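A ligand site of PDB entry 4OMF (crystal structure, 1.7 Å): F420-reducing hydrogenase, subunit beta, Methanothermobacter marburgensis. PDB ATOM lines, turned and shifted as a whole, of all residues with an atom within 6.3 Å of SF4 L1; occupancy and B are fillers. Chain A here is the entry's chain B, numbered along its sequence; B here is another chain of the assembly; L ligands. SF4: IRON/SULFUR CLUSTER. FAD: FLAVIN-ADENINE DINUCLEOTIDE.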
ATOM      1  N   PHE A  78      18.183 -30.447  -5.378  1.00  0.00           N
ATOM      2  CA  PHE A  78      17.388 -31.621  -5.724  1.00  0.00           C
ATOM      3  C   PHE A  78      17.920 -32.915  -5.139  1.00  0.00           C
ATOM      4  O   PHE A  78      19.119 -33.196  -5.197  1.00  0.00           O
ATOM      5  CB  PHE A  78      17.306 -31.792  -7.251  1.00  0.00           C
ATOM      6  CG  PHE A  78      16.901 -30.533  -7.976  1.00  0.00           C
ATOM      7  CD1 PHE A  78      17.663 -30.049  -9.027  1.00  0.00           C
ATOM      8  CD2 PHE A  78      15.744 -29.855  -7.623  1.00  0.00           C
ATOM      9  CE1 PHE A  78      17.293 -28.896  -9.708  1.00  0.00           C
ATOM     10  CE2 PHE A  78      15.373 -28.700  -8.290  1.00  0.00           C
ATOM     11  CZ  PHE A  78      16.153 -28.224  -9.338  1.00  0.00           C
ATOM     12  N   ILE A 102       9.625 -33.846   0.420  1.00  0.00           N
ATOM     13  CA  ILE A 102       9.048 -32.504   0.333  1.00  0.00           C
ATOM     14  C   ILE A 102       7.646 -32.632  -0.312  1.00  0.00           C
ATOM     15  O   ILE A 102       7.280 -33.705  -0.790  1.00  0.00           O
ATOM     16  CB  ILE A 102       9.983 -31.559  -0.461  1.00  0.00           C
ATOM     17  CG1 ILE A 102      10.334 -32.147  -1.838  1.00  0.00           C
ATOM     18  CG2 ILE A 102      11.264 -31.293   0.363  1.00  0.00           C
ATOM     19  CD1 ILE A 102      11.162 -31.176  -2.717  1.00  0.00           C
ATOM     20  N   PRO A 103       6.829 -31.570  -0.284  1.00  0.00           N
ATOM     21  CA  PRO A 103       5.428 -31.769  -0.712  1.00  0.00           C
ATOM     22  C   PRO A 103       5.246 -32.331  -2.140  1.00  0.00           C
ATOM     23  O   PRO A 103       4.420 -33.214  -2.308  1.00  0.00           O
ATOM     24  CB  PRO A 103       4.820 -30.374  -0.587  1.00  0.00           C
ATOM     25  CG  PRO A 103       5.571 -29.773   0.623  1.00  0.00           C
ATOM     26  CD  PRO A 103       7.014 -30.275   0.422  1.00  0.00           C
ATOM     27  N   CYS A 104       6.006 -31.857  -3.133  1.00  0.00           N
ATOM     28  CA  CYS A 104       5.776 -32.354  -4.494  1.00  0.00           C
ATOM     29  C   CYS A 104       6.147 -33.835  -4.613  1.00  0.00           C
ATOM     30  O   CYS A 104       5.520 -34.569  -5.364  1.00  0.00           O
ATOM     31  CB  CYS A 104       6.551 -31.532  -5.526  1.00  0.00           C
ATOM     32  SG  CYS A 104       8.324 -31.454  -5.210  1.00  0.00           S
ATOM     33  N   GLN A 105       7.155 -34.269  -3.871  1.00  0.00           N
ATOM     34  CA  GLN A 105       7.486 -35.692  -3.858  1.00  0.00           C
ATOM     35  C   GLN A 105       6.391 -36.487  -3.176  1.00  0.00           C
ATOM     36  O   GLN A 105       6.036 -37.580  -3.637  1.00  0.00           O
ATOM     37  CB  GLN A 105       8.825 -35.944  -3.168  1.00  0.00           C
ATOM     38  CG  GLN A 105      10.010 -35.482  -4.030  1.00  0.00           C
ATOM     39  CD  GLN A 105      11.305 -35.452  -3.256  1.00  0.00           C
ATOM     40  OE1 GLN A 105      11.358 -35.820  -2.070  1.00  0.00           O
ATOM     41  NE2 GLN A 105      12.357 -34.968  -3.898  1.00  0.00           N
ATOM     42  N   MET A 107       3.371 -35.804  -3.324  1.00  0.00           N
ATOM     43  CA  MET A 107       2.295 -35.909  -4.302  1.00  0.00           C
ATOM     44  C   MET A 107       2.494 -37.041  -5.317  1.00  0.00           C
ATOM     45  O   MET A 107       1.566 -37.779  -5.627  1.00  0.00           O
ATOM     46  CB  MET A 107       2.137 -34.576  -5.054  1.00  0.00           C
ATOM     47  CG  MET A 107       1.683 -33.475  -4.120  1.00  0.00           C
ATOM     48  SD  MET A 107       1.656 -31.873  -4.953  1.00  0.00           S
ATOM     49  CE  MET A 107       2.009 -30.794  -3.590  1.00  0.00           C
ATOM     50  N   CYS A 134       8.266 -27.028   2.570  1.00  0.00           N
ATOM     51  CA  CYS A 134       9.077 -26.499   1.468  1.00  0.00           C
ATOM     52  C   CYS A 134       8.444 -25.280   0.817  1.00  0.00           C
ATOM     53  O   CYS A 134       7.249 -25.291   0.524  1.00  0.00           O
ATOM     54  CB  CYS A 134       9.293 -27.579   0.421  1.00  0.00           C
ATOM     55  SG  CYS A 134      10.392 -27.048  -0.902  1.00  0.00           S
ATOM     56  N   MET A 135       9.251 -24.249   0.537  1.00  0.00           N
ATOM     57  CA  MET A 135       8.757 -23.057  -0.161  1.00  0.00           C
ATOM     58  C   MET A 135       9.361 -22.931  -1.573  1.00  0.00           C
ATOM     59  O   MET A 135       8.802 -22.282  -2.458  1.00  0.00           O
ATOM     60  CB  MET A 135       9.078 -21.792   0.655  1.00  0.00           C
ATOM     61  CG  MET A 135       8.451 -20.531   0.093  1.00  0.00           C
ATOM     62  SD  MET A 135       6.655 -20.508   0.284  1.00  0.00           S
ATOM     63  CE  MET A 135       6.503 -20.024   2.001  1.00  0.00           C
ATOM     64  N   GLU A 136      10.509 -23.556  -1.783  1.00  0.00           N
ATOM     65  CA  GLU A 136      11.208 -23.495  -3.064  1.00  0.00           C
ATOM     66  C   GLU A 136      12.371 -24.452  -3.033  1.00  0.00           C
ATOM     67  O   GLU A 136      12.863 -24.785  -1.955  1.00  0.00           O
ATOM     68  CB  GLU A 136      11.724 -22.078  -3.369  1.00  0.00           C
ATOM     69  CG  GLU A 136      12.757 -21.542  -2.380  1.00  0.00           C
ATOM     70  CD  GLU A 136      12.152 -20.716  -1.258  1.00  0.00           C
ATOM     71  OE1 GLU A 136      12.541 -20.926  -0.084  1.00  0.00           O
ATOM     72  OE2 GLU A 136      11.299 -19.846  -1.540  1.00  0.00           O
ATOM     73  N   ASN A 137      12.831 -24.897  -4.207  1.00  0.00           N
ATOM     74  CA  ASN A 137      14.088 -25.625  -4.279  1.00  0.00           C
ATOM     75  C   ASN A 137      14.967 -25.051  -5.408  1.00  0.00           C
ATOM     76  O   ASN A 137      14.469 -24.392  -6.308  1.00  0.00           O
ATOM     77  CB  ASN A 137      13.843 -27.129  -4.473  1.00  0.00           C
ATOM     78  CG  ASN A 137      14.976 -27.966  -3.908  1.00  0.00           C
ATOM     79  OD1 ASN A 137      15.972 -27.441  -3.430  1.00  0.00           O
ATOM     80  ND2 ASN A 137      14.816 -29.295  -3.941  1.00  0.00           N
ATOM     81  N   GLN A 189      13.952 -23.245  -9.122  1.00  0.00           N
ATOM     82  CA  GLN A 189      13.405 -23.861 -10.337  1.00  0.00           C
ATOM     83  C   GLN A 189      12.009 -23.275 -10.628  1.00  0.00           C
ATOM     84  O   GLN A 189      11.253 -22.986  -9.702  1.00  0.00           O
ATOM     85  CB  GLN A 189      13.367 -25.391 -10.234  1.00  0.00           C
ATOM     86  CG  GLN A 189      12.486 -25.916  -9.097  1.00  0.00           C
ATOM     87  CD  GLN A 189      12.338 -27.427  -9.087  1.00  0.00           C
ATOM     88  OE1 GLN A 189      12.831 -28.123  -9.978  1.00  0.00           O
ATOM     89  NE2 GLN A 189      11.674 -27.949  -8.057  1.00  0.00           N
ATOM     90  N   GLY A 191       9.391 -24.483 -11.766  1.00  0.00           N
ATOM     91  CA  GLY A 191       8.271 -25.363 -11.457  1.00  0.00           C
ATOM     92  C   GLY A 191       7.643 -25.108 -10.091  1.00  0.00           C
ATOM     93  O   GLY A 191       6.496 -25.467  -9.831  1.00  0.00           O
ATOM     94  N   CYS A 192       8.389 -24.458  -9.210  1.00  0.00           N
ATOM     95  CA  CYS A 192       7.899 -24.151  -7.872  1.00  0.00           C
ATOM     96  C   CYS A 192       6.818 -23.074  -7.880  1.00  0.00           C
ATOM     97  O   CYS A 192       6.093 -22.928  -6.912  1.00  0.00           O
ATOM     98  CB  CYS A 192       9.033 -23.712  -6.962  1.00  0.00           C
ATOM     99  SG  CYS A 192      10.200 -25.013  -6.583  1.00  0.00           S
ATOM    100  N   LYS A 193       6.714 -22.319  -8.987  1.00  0.00           N
ATOM    101  CA  LYS A 193       5.820 -21.168  -9.063  1.00  0.00           C
ATOM    102  C   LYS A 193       4.364 -21.514  -8.837  1.00  0.00           C
ATOM    103  O   LYS A 193       3.592 -20.675  -8.377  1.00  0.00           O
ATOM    104  CB  LYS A 193       5.929 -20.474 -10.436  1.00  0.00           C
ATOM    105  CG  LYS A 193       7.132 -19.602 -10.671  1.00  0.00           C
ATOM    106  CD  LYS A 193       7.167 -19.138 -12.145  1.00  0.00           C
ATOM    107  CE  LYS A 193       8.587 -18.776 -12.592  1.00  0.00           C
ATOM    108  NZ  LYS A 193       8.737 -18.529 -14.080  1.00  0.00           N
ATOM    109  N   CYS A 195       3.252 -24.232  -7.089  1.00  0.00           N
ATOM    110  CA  CYS A 195       3.105 -25.152  -5.974  1.00  0.00           C
ATOM    111  C   CYS A 195       2.256 -24.527  -4.839  1.00  0.00           C
ATOM    112  O   CYS A 195       2.562 -23.433  -4.348  1.00  0.00           O
ATOM    113  CB  CYS A 195       4.466 -25.558  -5.443  1.00  0.00           C
ATOM    114  SG  CYS A 195       4.351 -26.812  -4.120  1.00  0.00           S
ATOM    115  N   LYS A 196       1.194 -25.216  -4.424  1.00  0.00           N
ATOM    116  CA  LYS A 196       0.266 -24.688  -3.415  1.00  0.00           C
ATOM    117  C   LYS A 196       0.503 -25.264  -2.014  1.00  0.00           C
ATOM    118  O   LYS A 196      -0.098 -24.807  -1.034  1.00  0.00           O
ATOM    119  CB  LYS A 196      -1.200 -24.971  -3.804  1.00  0.00           C
ATOM    120  CG  LYS A 196      -1.645 -24.310  -5.108  1.00  0.00           C
ATOM    121  CD  LYS A 196      -2.666 -25.170  -5.879  1.00  0.00           C
ATOM    122  CE  LYS A 196      -4.073 -25.056  -5.307  1.00  0.00           C
ATOM    123  NZ  LYS A 196      -5.123 -25.565  -6.243  1.00  0.00           N
ATOM    124  N   ASP A 197       1.346 -26.275  -1.923  1.00  0.00           N
ATOM    125  CA  ASP A 197       1.454 -27.087  -0.723  1.00  0.00           C
ATOM    126  C   ASP A 197       2.725 -26.688   0.049  1.00  0.00           C
ATOM    127  O   ASP A 197       3.837 -26.994  -0.381  1.00  0.00           O
ATOM    128  CB  ASP A 197       1.469 -28.575  -1.127  1.00  0.00           C
ATOM    129  CG  ASP A 197       1.302 -29.544   0.049  1.00  0.00           C
ATOM    130  OD1 ASP A 197       1.623 -29.211   1.210  1.00  0.00           O
ATOM    131  OD2 ASP A 197       0.865 -30.688  -0.235  1.00  0.00           O
ATOM    132  N   LYS A 261       2.021 -18.717   0.242  1.00  0.00           N
ATOM    133  CA  LYS A 261       2.447 -19.629  -0.831  1.00  0.00           C
ATOM    134  C   LYS A 261       1.254 -19.925  -1.742  1.00  0.00           C
ATOM    135  O   LYS A 261       1.388 -19.946  -2.957  1.00  0.00           O
ATOM    136  CB  LYS A 261       3.027 -20.925  -0.277  1.00  0.00           C
ATOM    137  CG  LYS A 261       3.677 -21.806  -1.353  1.00  0.00           C
ATOM    138  CD  LYS A 261       4.211 -23.093  -0.761  1.00  0.00           C
ATOM    139  CE  LYS A 261       4.980 -23.881  -1.842  1.00  0.00           C
ATOM    140  NZ  LYS A 261       5.530 -25.158  -1.329  1.00  0.00           N
ATOM    141  N   ILE B 221       9.428 -30.578 -11.445  1.00  0.00           N
ATOM    142  CA  ILE B 221      10.014 -30.154 -10.168  1.00  0.00           C
ATOM    143  C   ILE B 221      10.984 -31.180  -9.583  1.00  0.00           C
ATOM    144  O   ILE B 221      11.340 -31.110  -8.403  1.00  0.00           O
ATOM    145  CB  ILE B 221       8.898 -29.807  -9.171  1.00  0.00           C
ATOM    146  CG1 ILE B 221       7.720 -30.781  -9.243  1.00  0.00           C
ATOM    147  CG2 ILE B 221       8.361 -28.415  -9.510  1.00  0.00           C
ATOM    148  CD1 ILE B 221       8.034 -32.231  -8.841  1.00  0.00           C
ATOM    149  N   ARG B 261       2.689 -34.052 -12.214  1.00  0.00           N
ATOM    150  CA  ARG B 261       2.375 -32.801 -12.900  1.00  0.00           C
ATOM    151  C   ARG B 261       1.643 -33.023 -14.231  1.00  0.00           C
ATOM    152  O   ARG B 261       1.323 -32.065 -14.926  1.00  0.00           O
ATOM    153  CB  ARG B 261       3.676 -31.972 -13.106  1.00  0.00           C
ATOM    154  CG  ARG B 261       4.254 -31.412 -11.824  1.00  0.00           C
ATOM    155  CD  ARG B 261       3.518 -30.145 -11.453  1.00  0.00           C
ATOM    156  NE  ARG B 261       3.878 -29.534 -10.185  1.00  0.00           N
ATOM    157  CZ  ARG B 261       4.569 -28.400 -10.067  1.00  0.00           C
ATOM    158  NH1 ARG B 261       5.063 -27.781 -11.147  1.00  0.00           N
ATOM    159  NH2 ARG B 261       4.769 -27.878  -8.876  1.00  0.00           N
HETATM  160 FE1  SF4 L   1       8.451 -29.115  -4.725  1.00  0.00          FE
HETATM  161 FE2  SF4 L   1       6.662 -27.243  -4.168  1.00  0.00          FE
HETATM  162 FE3  SF4 L   1       8.943 -26.546  -5.382  1.00  0.00          FE
HETATM  163 FE4  SF4 L   1       9.041 -27.326  -2.805  1.00  0.00          FE
HETATM  164  S1  SF4 L   1       7.970 -25.431  -3.615  1.00  0.00           S
HETATM  165  S2  SF4 L   1      10.437 -28.060  -4.507  1.00  0.00           S
HETATM  166  S3  SF4 L   1       7.368 -28.834  -2.701  1.00  0.00           S
HETATM  167  S4  SF4 L   1       7.296 -27.872  -6.284  1.00  0.00           S
HETATM  168  PA  FAD L   2      16.895 -34.172  10.152  1.00  0.00           P
HETATM  169  O1A FAD L   2      17.920 -33.085   9.966  1.00  0.00           O
HETATM  170  O2A FAD L   2      16.947 -35.166  11.268  1.00  0.00           O
HETATM  171  O5B FAD L   2      16.841 -34.997   8.790  1.00  0.00           O
HETATM  172  C5B FAD L   2      16.599 -34.232   7.609  1.00  0.00           C
HETATM  173  C4B FAD L   2      16.014 -35.177   6.557  1.00  0.00           C
HETATM  174  O4B FAD L   2      15.703 -34.444   5.373  1.00  0.00           O
HETATM  175  C3B FAD L   2      17.032 -36.253   6.186  1.00  0.00           C
HETATM  176  O3B FAD L   2      16.461 -37.563   6.223  1.00  0.00           O
HETATM  177  C2B FAD L   2      17.405 -35.884   4.750  1.00  0.00           C
HETATM  178  O2B FAD L   2      17.663 -37.073   3.978  1.00  0.00           O
HETATM  179  C1B FAD L   2      16.186 -35.145   4.245  1.00  0.00           C
HETATM  180  N9A FAD L   2      16.578 -34.199   3.188  1.00  0.00           N
HETATM  181  C8A FAD L   2      17.537 -33.264   3.285  1.00  0.00           C
HETATM  182  N7A FAD L   2      17.632 -32.548   2.138  1.00  0.00           N
HETATM  183  C5A FAD L   2      16.692 -33.054   1.284  1.00  0.00           C
HETATM  184  C6A FAD L   2      16.265 -32.780  -0.101  1.00  0.00           C
HETATM  185  N6A FAD L   2      16.862 -31.812  -0.854  1.00  0.00           N
HETATM  186  N1A FAD L   2      15.264 -33.522  -0.597  1.00  0.00           N
HETATM  187  C2A FAD L   2      14.672 -34.519   0.109  1.00  0.00           C
HETATM  188  N3A FAD L   2      15.012 -34.831   1.383  1.00  0.00           N
HETATM  189  C4A FAD L   2      16.008 -34.134   1.991  1.00  0.00           C
HETATM  190  N1  FAD L   2      11.435 -26.076   6.485  1.00  0.00           N
HETATM  191  C2  FAD L   2      10.485 -25.085   6.744  1.00  0.00           C
HETATM  192  O2  FAD L   2      10.119 -24.899   7.930  1.00  0.00           O
HETATM  193  N3  FAD L   2      10.016 -24.309   5.703  1.00  0.00           N
HETATM  194  C4  FAD L   2      10.421 -24.544   4.406  1.00  0.00           C
HETATM  195  O4  FAD L   2       9.937 -23.839   3.479  1.00  0.00           O
HETATM  196  C4X FAD L   2      11.769 -25.024   4.243  1.00  0.00           C
HETATM  197  N5  FAD L   2      12.237 -25.154   2.839  1.00  0.00           N
HETATM  198  C5X FAD L   2      12.753 -26.496   2.533  1.00  0.00           C
HETATM  199  C6  FAD L   2      13.143 -26.680   1.199  1.00  0.00           C
HETATM  200  C7  FAD L   2      13.847 -27.839   0.842  1.00  0.00           C
HETATM  201  C7M FAD L   2      14.271 -28.062  -0.613  1.00  0.00           C
HETATM  202  C8  FAD L   2      14.155 -28.771   1.834  1.00  0.00           C
HETATM  203  C8M FAD L   2      14.911 -30.055   1.567  1.00  0.00           C
HETATM  204  C9  FAD L   2      13.768 -28.580   3.174  1.00  0.00           C
HETATM  205  C9A FAD L   2      13.142 -27.385   3.557  1.00  0.00           C
HETATM  206  N10 FAD L   2      12.675 -27.229   4.886  1.00  0.00           N
HETATM  207  C10 FAD L   2      12.114 -26.030   5.290  1.00  0.00           C
HETATM  208  C1' FAD L   2      12.674 -28.309   5.885  1.00  0.00           C
HETATM  209  C2' FAD L   2      13.866 -28.316   6.796  1.00  0.00           C
HETATM  210  O2' FAD L   2      14.933 -27.600   6.350  1.00  0.00           O
HETATM  211  C3' FAD L   2      14.117 -29.533   7.343  1.00  0.00           C
HETATM  212  O3' FAD L   2      14.624 -30.422   6.461  1.00  0.00           O
HETATM  213  C4' FAD L   2      13.055 -30.093   8.272  1.00  0.00           C
HETATM  214  O4' FAD L   2      12.698 -29.159   9.314  1.00  0.00           O
HETATM  215  C5' FAD L   2      13.513 -31.423   8.875  1.00  0.00           C
HETATM  216  O5' FAD L   2      14.465 -31.182   9.897  1.00  0.00           O
HETATM  217  P   FAD L   2      14.801 -32.290  10.998  1.00  0.00           P
HETATM  218  O1P FAD L   2      13.477 -32.774  11.547  1.00  0.00           O
HETATM  219  O2P FAD L   2      15.824 -31.759  11.964  1.00  0.00           O
HETATM  220  O3P FAD L   2      15.424 -33.497  10.093  1.00  0.00           O
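SG of Cys 195 binds FE2 of SF4 L1, at 2.4 Å.
The backbone NH (N) of Met 135 lies within hydrogen-bond range of an oxygen (O4) of FAD L2, at 3.0 Å.
S4 of SF4 L1 lies close to NH2 of Arg 261 of chain B, at 3.6 Å.
FE4 of SF4 L1 is bound by SG of Cys 134, at 2.4 Å.
NE2 of Gln 189 lies close to S2 of SF4 L1, 3.8 Å away.
SG of Cys 192 is bound to FE3 of SF4 L1, at 2.3 Å.
The side-chain amino group (NZ) of Lys 261 of chain A sits close to a sulfur (S1) of SF4 L1, 3.4 Å away.
The backbone NH (N) of Glu 136 sits close to a sulfur (S1) of SF4 L1 (3.6 Å).
The backbone NH of Cys 104 sits close to a sulfur (S3) of SF4 L1, 3.3 Å away.
The side-chain sulfur (SG) of Cys 104 binds an iron atom (FE1) of SF4 L1 (2.4 Å).
NZ of Lys 261 of chain A lies close to SG of Cys 195 (3.5 Å).
The backbone NH (N) of Asp 197 lies close to the side-chain sulfur (SG) of Cys 195, at 3.8 Å.
The side-chain sulfur of Cys 192 lies close to the side-chain amide nitrogen of Gln 189.
The side-chain amino group (NZ) of Lys 261 of chain A sits at hydrogen-bond distance from the backbone carbonyl oxygen (O) of Asp 197, 2.7 Å away.
The backbone NH (N) of Gln 189 is in hydrogen-bond range of the backbone carbonyl oxygen (O) of Asn 137.
The side-chain sulfur (SG) of Cys 134 lies close to the backbone carbonyl oxygen (O) of Glu 136, 3.5 Å away.
The backbone carbonyl oxygen of Cys 134 lies within hydrogen-bond range of the side-chain amino group of Lys 261 of chain A (2.5 Å).
NH1 of Arg 261 of chain B sits at hydrogen-bond distance from O of Gly 191 (3.0 Å).
The backbone nitrogen (N) of Pro 103 sits close to a sulfur (S3) of SF4 L1, at 3.7 Å.
The backbone carbonyl oxygen (O) of Met 135 lies close to a sulfur (S1) of SF4 L1 (3.5 Å).
Residues that only touch SF4 L1: Ile 102, Asn 137 and Ile 221 of chain B.
Of the 20 residues printed, 13 come within 4 Å of SF4 L1.
The nearest printed residue that does not touch SF4 L1 is Gly 191 (4.4 Å).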
